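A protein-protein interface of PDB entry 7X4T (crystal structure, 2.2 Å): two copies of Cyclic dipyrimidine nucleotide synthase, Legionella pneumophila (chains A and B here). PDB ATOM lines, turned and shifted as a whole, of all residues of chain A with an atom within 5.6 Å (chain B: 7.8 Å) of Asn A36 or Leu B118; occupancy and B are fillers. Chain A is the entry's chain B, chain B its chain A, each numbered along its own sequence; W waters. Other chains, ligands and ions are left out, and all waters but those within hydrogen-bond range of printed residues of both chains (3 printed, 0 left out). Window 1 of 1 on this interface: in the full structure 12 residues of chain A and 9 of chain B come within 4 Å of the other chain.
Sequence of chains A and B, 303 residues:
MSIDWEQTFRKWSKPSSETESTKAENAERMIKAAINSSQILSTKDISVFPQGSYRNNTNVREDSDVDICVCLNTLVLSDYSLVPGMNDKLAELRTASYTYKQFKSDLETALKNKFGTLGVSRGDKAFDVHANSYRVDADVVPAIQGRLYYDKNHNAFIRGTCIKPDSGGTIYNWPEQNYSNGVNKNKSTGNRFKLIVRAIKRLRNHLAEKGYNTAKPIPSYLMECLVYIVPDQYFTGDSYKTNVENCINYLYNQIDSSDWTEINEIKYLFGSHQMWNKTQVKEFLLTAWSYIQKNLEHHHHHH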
ATOM      1  N   ILE A  31     -32.637   2.743  14.047  1.00  0.00           N
ATOM      2  CA  ILE A  31     -32.346   4.162  13.871  1.00  0.00           C
ATOM      3  C   ILE A  31     -31.504   4.691  15.028  1.00  0.00           C
ATOM      4  O   ILE A  31     -30.583   5.501  14.834  1.00  0.00           O
ATOM      5  CB  ILE A  31     -33.653   4.948  13.680  1.00  0.00           C
ATOM      6  CG1 ILE A  31     -34.252   4.565  12.324  1.00  0.00           C
ATOM      7  CG2 ILE A  31     -33.410   6.454  13.790  1.00  0.00           C
ATOM      8  CD1 ILE A  31     -35.723   4.675  12.276  1.00  0.00           C
ATOM      9  N   LYS A  32     -31.786   4.233  16.245  1.00  0.00           N
ATOM     10  CA  LYS A  32     -30.938   4.602  17.369  1.00  0.00           C
ATOM     11  C   LYS A  32     -29.502   4.137  17.143  1.00  0.00           C
ATOM     12  O   LYS A  32     -28.551   4.865  17.451  1.00  0.00           O
ATOM     13  CB  LYS A  32     -31.516   4.015  18.657  1.00  0.00           C
ATOM     14  CG  LYS A  32     -31.156   4.771  19.904  1.00  0.00           C
ATOM     15  CD  LYS A  32     -32.034   4.353  21.083  1.00  0.00           C
ATOM     16  CE  LYS A  32     -33.475   4.758  20.866  1.00  0.00           C
ATOM     17  NZ  LYS A  32     -34.275   4.680  22.118  1.00  0.00           N
ATOM     18  N   ALA A  33     -29.321   2.938  16.576  1.00  0.00           N
ATOM     19  CA  ALA A  33     -27.971   2.454  16.295  1.00  0.00           C
ATOM     20  C   ALA A  33     -27.281   3.320  15.248  1.00  0.00           C
ATOM     21  O   ALA A  33     -26.080   3.597  15.357  1.00  0.00           O
ATOM     22  CB  ALA A  33     -28.015   0.992  15.838  1.00  0.00           C
ATOM     23  N   ALA A  34     -28.022   3.756  14.223  1.00  0.00           N
ATOM     24  CA  ALA A  34     -27.446   4.681  13.247  1.00  0.00           C
ATOM     25  C   ALA A  34     -26.986   5.973  13.912  1.00  0.00           C
ATOM     26  O   ALA A  34     -25.910   6.494  13.594  1.00  0.00           O
ATOM     27  CB  ALA A  34     -28.454   4.999  12.138  1.00  0.00           C
ATOM     28  N   ILE A  35     -27.795   6.517  14.823  1.00  0.00           N
ATOM     29  CA  ILE A  35     -27.407   7.760  15.489  1.00  0.00           C
ATOM     30  C   ILE A  35     -26.184   7.535  16.374  1.00  0.00           C
ATOM     31  O   ILE A  35     -25.266   8.366  16.413  1.00  0.00           O
ATOM     32  CB  ILE A  35     -28.576   8.350  16.296  1.00  0.00           C
ATOM     33  CG1 ILE A  35     -29.810   8.527  15.409  1.00  0.00           C
ATOM     34  CG2 ILE A  35     -28.176   9.704  16.842  1.00  0.00           C
ATOM     35  CD1 ILE A  35     -29.552   9.323  14.183  1.00  0.00           C
ATOM     36  N   ASN A  36     -26.166   6.428  17.121  1.00  0.00           N
ATOM     37  CA  ASN A  36     -25.041   6.125  18.004  1.00  0.00           C
ATOM     38  C   ASN A  36     -23.763   5.851  17.236  1.00  0.00           C
ATOM     39  O   ASN A  36     -22.676   5.962  17.812  1.00  0.00           O
ATOM     40  CB  ASN A  36     -25.363   4.929  18.902  1.00  0.00           C
ATOM     41  CG  ASN A  36     -26.276   5.302  20.042  1.00  0.00           C
ATOM     42  OD1 ASN A  36     -26.151   6.388  20.602  1.00  0.00           O
ATOM     43  ND2 ASN A  36     -27.217   4.428  20.375  1.00  0.00           N
ATOM     44  N   SER A  37     -23.866   5.474  15.964  1.00  0.00           N
ATOM     45  CA  SER A  37     -22.675   5.294  15.147  1.00  0.00           C
ATOM     46  C   SER A  37     -22.178   6.603  14.553  1.00  0.00           C
ATOM     47  O   SER A  37     -21.056   6.640  14.040  1.00  0.00           O
ATOM     48  CB  SER A  37     -22.944   4.289  14.019  1.00  0.00           C
ATOM     49  OG  SER A  37     -23.164   2.987  14.543  1.00  0.00           O
ATOM     50  N   SER A  38     -22.966   7.672  14.641  1.00  0.00           N
ATOM     51  CA  SER A  38     -22.591   8.958  14.068  1.00  0.00           C
ATOM     52  C   SER A  38     -21.649   9.696  15.009  1.00  0.00           C
ATOM     53  O   SER A  38     -22.011  10.000  16.149  1.00  0.00           O
ATOM     54  CB  SER A  38     -23.834   9.799  13.795  1.00  0.00           C
ATOM     55  OG  SER A  38     -23.488  11.164  13.611  1.00  0.00           O
ATOM     56  N   LEU A  41     -23.523  13.034  15.819  1.00  0.00           N
ATOM     57  CA  LEU A  41     -24.799  13.024  16.535  1.00  0.00           C
ATOM     58  C   LEU A  41     -24.763  12.220  17.831  1.00  0.00           C
ATOM     59  O   LEU A  41     -25.559  12.492  18.739  1.00  0.00           O
ATOM     60  CB  LEU A  41     -25.903  12.477  15.622  1.00  0.00           C
ATOM     61  CG  LEU A  41     -26.263  13.337  14.409  1.00  0.00           C
ATOM     62  CD1 LEU A  41     -27.402  12.714  13.615  1.00  0.00           C
ATOM     63  CD2 LEU A  41     -26.628  14.751  14.843  1.00  0.00           C
ATOM     64  N   SER A  42     -23.867  11.236  17.945  1.00  0.00           N
ATOM     65  CA  SER A  42     -23.895  10.344  19.106  1.00  0.00           C
ATOM     66  C   SER A  42     -23.636  11.059  20.422  1.00  0.00           C
ATOM     67  O   SER A  42     -23.988  10.521  21.474  1.00  0.00           O
ATOM     68  CB  SER A  42     -22.872   9.222  18.949  1.00  0.00           C
ATOM     69  OG  SER A  42     -21.551   9.740  18.950  1.00  0.00           O
ATOM     70  N   THR A  43     -23.030  12.244  20.395  1.00  0.00           N
ATOM     71  CA  THR A  43     -22.765  13.009  21.606  1.00  0.00           C
ATOM     72  C   THR A  43     -23.874  13.997  21.964  1.00  0.00           C
ATOM     73  O   THR A  43     -23.798  14.621  23.026  1.00  0.00           O
ATOM     74  CB  THR A  43     -21.424  13.750  21.486  1.00  0.00           C
ATOM     75  OG1 THR A  43     -21.427  14.583  20.320  1.00  0.00           O
ATOM     76  CG2 THR A  43     -20.277  12.752  21.367  1.00  0.00           C
ATOM     77  N   LYS A  44     -24.889  14.160  21.118  1.00  0.00           N
ATOM     78  CA  LYS A  44     -25.940  15.142  21.346  1.00  0.00           C
ATOM     79  C   LYS A  44     -27.113  14.551  22.130  1.00  0.00           C
ATOM     80  O   LYS A  44     -27.269  13.333  22.245  1.00  0.00           O
ATOM     81  CB  LYS A  44     -26.423  15.725  20.015  1.00  0.00           C
ATOM     82  CG  LYS A  44     -25.312  16.371  19.196  1.00  0.00           C
ATOM     83  CD  LYS A  44     -25.848  17.033  17.928  1.00  0.00           C
ATOM     84  CE  LYS A  44     -24.729  17.710  17.134  1.00  0.00           C
ATOM     85  NZ  LYS A  44     -24.078  18.809  17.915  1.00  0.00           N
ATOM     86  N   ILE A  46     -30.468  13.609  22.057  1.00  0.00           N
ATOM     87  CA  ILE A  46     -31.390  13.253  20.987  1.00  0.00           C
ATOM     88  C   ILE A  46     -32.308  12.146  21.483  1.00  0.00           C
ATOM     89  O   ILE A  46     -31.839  11.149  22.042  1.00  0.00           O
ATOM     90  CB  ILE A  46     -30.636  12.797  19.721  1.00  0.00           C
ATOM     91  CG1 ILE A  46     -29.884  13.970  19.086  1.00  0.00           C
ATOM     92  CG2 ILE A  46     -31.600  12.183  18.712  1.00  0.00           C
ATOM     93  CD1 ILE A  46     -28.895  13.552  18.005  1.00  0.00           C
ATOM     94  N   SER A  47     -33.608  12.310  21.263  1.00  0.00           N
ATOM     95  CA  SER A  47     -34.587  11.265  21.542  1.00  0.00           C
ATOM     96  C   SER A  47     -35.021  10.617  20.235  1.00  0.00           C
ATOM     97  O   SER A  47     -35.364  11.314  19.279  1.00  0.00           O
ATOM     98  CB  SER A  47     -35.809  11.819  22.280  1.00  0.00           C
ATOM     99  OG  SER A  47     -35.447  12.446  23.503  1.00  0.00           O
ATOM    100  N   VAL A  48     -34.970   9.293  20.182  1.00  0.00           N
ATOM    101  CA  VAL A  48     -35.429   8.530  19.027  1.00  0.00           C
ATOM    102  C   VAL A  48     -36.629   7.716  19.484  1.00  0.00           C
ATOM    103  O   VAL A  48     -36.482   6.804  20.306  1.00  0.00           O
ATOM    104  CB  VAL A  48     -34.330   7.620  18.469  1.00  0.00           C
ATOM    105  CG1 VAL A  48     -34.864   6.826  17.295  1.00  0.00           C
ATOM    106  CG2 VAL A  48     -33.094   8.438  18.070  1.00  0.00           C
ATOM    107  N   LYS B 112     -32.268   6.661  31.612  1.00  0.00           N
ATOM    108  CA  LYS B 112     -32.200   7.765  30.659  1.00  0.00           C
ATOM    109  C   LYS B 112     -31.454   8.953  31.251  1.00  0.00           C
ATOM    110  O   LYS B 112     -30.638   9.580  30.567  1.00  0.00           O
ATOM    111  CB  LYS B 112     -33.613   8.179  30.248  1.00  0.00           C
ATOM    112  CG  LYS B 112     -34.347   7.199  29.334  1.00  0.00           C
ATOM    113  CD  LYS B 112     -35.723   7.770  28.955  1.00  0.00           C
ATOM    114  CE  LYS B 112     -36.391   6.980  27.837  1.00  0.00           C
ATOM    115  NZ  LYS B 112     -37.784   7.440  27.545  1.00  0.00           N
ATOM    116  N   PHE B 115     -27.583   7.760  31.289  1.00  0.00           N
ATOM    117  CA  PHE B 115     -26.928   7.444  30.028  1.00  0.00           C
ATOM    118  C   PHE B 115     -27.428   8.273  28.857  1.00  0.00           C
ATOM    119  O   PHE B 115     -26.891   8.140  27.755  1.00  0.00           O
ATOM    120  CB  PHE B 115     -27.108   5.956  29.704  1.00  0.00           C
ATOM    121  CG  PHE B 115     -26.590   5.028  30.770  1.00  0.00           C
ATOM    122  CD1 PHE B 115     -25.227   4.923  31.020  1.00  0.00           C
ATOM    123  CD2 PHE B 115     -27.465   4.253  31.516  1.00  0.00           C
ATOM    124  CE1 PHE B 115     -24.746   4.065  31.998  1.00  0.00           C
ATOM    125  CE2 PHE B 115     -26.996   3.394  32.504  1.00  0.00           C
ATOM    126  CZ  PHE B 115     -25.635   3.297  32.746  1.00  0.00           C
ATOM    127  N   GLY B 116     -28.424   9.124  29.058  1.00  0.00           N
ATOM    128  CA  GLY B 116     -28.983   9.840  27.917  1.00  0.00           C
ATOM    129  C   GLY B 116     -30.061   9.036  27.215  1.00  0.00           C
ATOM    130  O   GLY B 116     -30.096   7.807  27.263  1.00  0.00           O
ATOM    131  N   THR B 117     -30.978   9.756  26.562  1.00  0.00           N
ATOM    132  CA  THR B 117     -32.084   9.102  25.863  1.00  0.00           C
ATOM    133  C   THR B 117     -31.598   8.226  24.711  1.00  0.00           C
ATOM    134  O   THR B 117     -32.199   7.181  24.436  1.00  0.00           O
ATOM    135  CB  THR B 117     -33.083  10.148  25.356  1.00  0.00           C
ATOM    136  OG1 THR B 117     -32.392  11.153  24.606  1.00  0.00           O
ATOM    137  CG2 THR B 117     -33.802  10.814  26.522  1.00  0.00           C
ATOM    138  N   LEU B 118     -30.517   8.625  24.026  1.00  0.00           N
ATOM    139  CA  LEU B 118     -30.001   7.824  22.916  1.00  0.00           C
ATOM    140  C   LEU B 118     -29.512   6.455  23.356  1.00  0.00           C
ATOM    141  O   LEU B 118     -29.475   5.527  22.542  1.00  0.00           O
ATOM    142  CB  LEU B 118     -28.842   8.531  22.213  1.00  0.00           C
ATOM    143  CG  LEU B 118     -29.115   9.357  20.976  1.00  0.00           C
ATOM    144  CD1 LEU B 118     -27.792   9.856  20.422  1.00  0.00           C
ATOM    145  CD2 LEU B 118     -29.803   8.454  19.977  1.00  0.00           C
ATOM    146  N   GLY B 119     -29.114   6.309  24.615  1.00  0.00           N
ATOM    147  CA  GLY B 119     -28.516   5.067  25.049  1.00  0.00           C
ATOM    148  C   GLY B 119     -29.436   4.049  25.676  1.00  0.00           C
ATOM    149  O   GLY B 119     -28.949   3.016  26.142  1.00  0.00           O
ATOM    150  N   VAL B 120     -30.744   4.297  25.721  1.00  0.00           N
ATOM    151  CA  VAL B 120     -31.676   3.438  26.444  1.00  0.00           C
ATOM    152  C   VAL B 120     -32.875   3.157  25.556  1.00  0.00           C
ATOM    153  O   VAL B 120     -33.470   4.082  24.998  1.00  0.00           O
ATOM    154  CB  VAL B 120     -32.140   4.078  27.770  1.00  0.00           C
ATOM    155  CG1 VAL B 120     -33.116   3.160  28.487  1.00  0.00           C
ATOM    156  CG2 VAL B 120     -30.951   4.409  28.659  1.00  0.00           C
ATOM    157  N   SER B 121     -33.233   1.881  25.430  1.00  0.00           N
ATOM    158  CA  SER B 121     -34.429   1.487  24.703  1.00  0.00           C
ATOM    159  C   SER B 121     -35.222   0.517  25.555  1.00  0.00           C
ATOM    160  O   SER B 121     -34.666  -0.460  26.070  1.00  0.00           O
ATOM    161  CB  SER B 121     -34.079   0.853  23.358  1.00  0.00           C
ATOM    162  OG  SER B 121     -35.222   0.250  22.775  1.00  0.00           O
ATOM    163  N   ASP B 128     -32.533  -2.294  26.713  1.00  0.00           N
ATOM    164  CA  ASP B 128     -31.313  -2.408  25.931  1.00  0.00           C
ATOM    165  C   ASP B 128     -30.552  -1.093  26.083  1.00  0.00           C
ATOM    166  O   ASP B 128     -31.060  -0.031  25.703  1.00  0.00           O
ATOM    167  CB  ASP B 128     -31.670  -2.714  24.474  1.00  0.00           C
ATOM    168  CG  ASP B 128     -30.489  -3.209  23.657  1.00  0.00           C
ATOM    169  OD1 ASP B 128     -29.668  -4.001  24.174  1.00  0.00           O
ATOM    170  OD2 ASP B 128     -30.392  -2.808  22.474  1.00  0.00           O
ATOM    171  N   VAL B 129     -29.359  -1.152  26.670  1.00  0.00           N
ATOM    172  CA  VAL B 129     -28.580   0.037  27.003  1.00  0.00           C
ATOM    173  C   VAL B 129     -27.303   0.029  26.178  1.00  0.00           C
ATOM    174  O   VAL B 129     -26.509  -0.918  26.260  1.00  0.00           O
ATOM    175  CB  VAL B 129     -28.248   0.101  28.499  1.00  0.00           C
ATOM    176  CG1 VAL B 129     -27.314   1.280  28.777  1.00  0.00           C
ATOM    177  CG2 VAL B 129     -29.533   0.208  29.330  1.00  0.00           C
ATOM    178  N   HIS B 130     -27.089   1.095  25.406  1.00  0.00           N
ATOM    179  CA  HIS B 130     -25.868   1.238  24.616  1.00  0.00           C
ATOM    180  C   HIS B 130     -25.421   2.688  24.754  1.00  0.00           C
ATOM    181  O   HIS B 130     -25.879   3.562  24.013  1.00  0.00           O
ATOM    182  CB  HIS B 130     -26.105   0.834  23.167  1.00  0.00           C
ATOM    183  CG  HIS B 130     -26.503  -0.599  23.024  1.00  0.00           C
ATOM    184  ND1 HIS B 130     -25.587  -1.629  23.041  1.00  0.00           N
ATOM    185  CD2 HIS B 130     -27.722  -1.181  22.923  1.00  0.00           C
ATOM    186  CE1 HIS B 130     -26.222  -2.783  22.932  1.00  0.00           C
ATOM    187  NE2 HIS B 130     -27.519  -2.539  22.859  1.00  0.00           N
ATOM    188  N   ALA B 131     -24.495   2.923  25.677  1.00  0.00           N
ATOM    189  CA  ALA B 131     -24.082   4.263  26.075  1.00  0.00           C
ATOM    190  C   ALA B 131     -22.589   4.392  25.798  1.00  0.00           C
ATOM    191  O   ALA B 131     -21.757   3.895  26.569  1.00  0.00           O
ATOM    192  CB  ALA B 131     -24.404   4.496  27.549  1.00  0.00           C
ATOM    193  N   ASN B 132     -22.264   5.085  24.700  1.00  0.00           N
ATOM    194  CA  ASN B 132     -20.870   5.228  24.295  1.00  0.00           C
ATOM    195  C   ASN B 132     -20.075   6.039  25.301  1.00  0.00           C
ATOM    196  O   ASN B 132     -18.890   5.759  25.509  1.00  0.00           O
ATOM    197  CB  ASN B 132     -20.778   5.886  22.913  1.00  0.00           C
ATOM    198  CG  ASN B 132     -19.331   6.049  22.429  1.00  0.00           C
ATOM    199  OD1 ASN B 132     -18.508   5.134  22.557  1.00  0.00           O
ATOM    200  ND2 ASN B 132     -19.017   7.223  21.878  1.00  0.00           N
ATOM    201  N   SER B 133     -20.704   7.029  25.945  1.00  0.00           N
ATOM    202  CA  SER B 133     -19.958   7.894  26.857  1.00  0.00           C
ATOM    203  C   SER B 133     -19.389   7.099  28.025  1.00  0.00           C
ATOM    204  O   SER B 133     -18.256   7.342  28.457  1.00  0.00           O
ATOM    205  CB  SER B 133     -20.845   9.033  27.365  1.00  0.00           C
ATOM    206  OG  SER B 133     -21.779   8.552  28.317  1.00  0.00           O
ATOM    207  N   ASP B 137     -22.631  -1.558  27.319  1.00  0.00           N
ATOM    208  CA  ASP B 137     -23.579  -2.282  26.475  1.00  0.00           C
ATOM    209  C   ASP B 137     -24.193  -3.372  27.340  1.00  0.00           C
ATOM    210  O   ASP B 137     -23.513  -4.338  27.706  1.00  0.00           O
ATOM    211  CB  ASP B 137     -22.901  -2.872  25.231  1.00  0.00           C
ATOM    212  CG  ASP B 137     -22.324  -1.794  24.315  1.00  0.00           C
ATOM    213  OD1 ASP B 137     -23.105  -1.117  23.616  1.00  0.00           O
ATOM    214  OD2 ASP B 137     -21.090  -1.618  24.297  1.00  0.00           O
HETATM  215  O   HOH W   1     -20.838   9.191  21.701  1.00  0.00           O
HETATM  216  O   HOH W   2     -28.872   2.892  22.290  1.00  0.00           O
HETATM  217  O   HOH W   3     -34.411   7.866  22.594  1.00  0.00           O
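Hydrophobic or aromatic side chains of chain B within 4 Å of the printed part of chain A: Leu B118. Printed residues of chain A that touch a printed residue of chain B: Lys A32, Ile A35, Asn A36, Leu A41, Lys A44, Ile A46, Ser A47 and Val A48. Among the printed residues, 12 pairs touch across the chains. Among the printed residues, no Asp or Glu carboxylate lies within 4 Å of a Lys or Arg side-chain nitrogen of the other chain.
No position is printed for both chains.
Among the printed residues, pairs that only touch across the chains: Lys A32 with Thr B117 (3.99 Å), Lys A32 with Leu B118 (3.2 Å), Ile A35 with Leu B118 (3.6 Å), Asn A36 with His B130 (3.97 Å), Leu A41 with Leu B118 (3.8 Å), Lys A44 with Leu B118 (3.96 Å) and Val A48 with Leu B118 (3.8 Å).
OG1 of Thr B117 sits at hydrogen-bond distance from O of Ile A46 (2.6 Å). OG of Ser A47 is in hydrogen-bond range of OG1 of Thr B117 (3.5 Å). The backbone carbonyl oxygen (O) of Leu B118 is in hydrogen-bond range of the side-chain amide nitrogen (ND2) of Asn A36 (3.3 Å). The backbone carbonyl oxygen (O) of Ile A46 lies close to the backbone NH (N) of Leu B118, 3.5 Å away. The backbone carbonyl oxygen of Val B120 sits at hydrogen-bond distance from the side-chain amino group of Lys A32, 3.0 Å away.
The backbone NH (N) of His B130 is in hydrogen-bond range of the backbone carbonyl oxygen (O) of Gly B119, at 2.8 Å. The side-chain carboxylate (OD2) of Asp B128 lies within hydrogen-bond range of a ring nitrogen (NE2) of His B130, at 2.9 Å. ND1 of His B130 lies within hydrogen-bond range of OD1 of Asp B137 (2.6 Å). O of Lys A32 is in hydrogen-bond range of ND2 of Asn A36, 3.2 Å away. OG of Ser A38 is in hydrogen-bond range of N of Leu A41 (2.9 Å).
Water W1 bridges the side-chain amide nitrogen (ND2) of Asn B132 (2.7 Å) and the side-chain hydroxyl (OG) of Ser A42 (2.9 Å). Water W2 lies within hydrogen-bond range of the backbone carbonyl oxygen (O) of Leu B118 (2.7 Å) and the side-chain amide nitrogen (ND2) of Asn A36 (3.0 Å). Water W3 lies within hydrogen-bond range of the backbone NH of Val A48, the backbone carbonyl oxygen of Thr B117 and the side-chain amino group of Lys A32.
Ile A31 touches none of the printed residues of chain B. Of the printed residues of chain B, Ile A35 touches Leu B118 (3.6 Å). Asn A36 touches just these residues of chain B: Leu B118 (3.3 Å) and His B130 (3.97 Å). Printed residues of chain B within 4 Å of Lys A44: Leu B118. Of the printed residues of chain A, Leu B118 touches Lys A32 (3.2 Å), Ile A35 (3.6 Å), Asn A36 (3.3 Å), Leu A41 (3.8 Å), Lys A44 (3.96 Å), Ile A46 (3.4 Å) and Val A48 (3.8 Å). Of the printed residues of chain A, Val B120 touches Lys A32 (3.0 Å). The nearest residue of chain B that does not touch Asn A36 is Gly B119 (4.9 Å). The nearest printed residue of chain A that does not touch Leu B118 is Ser A42 (4.002 Å).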
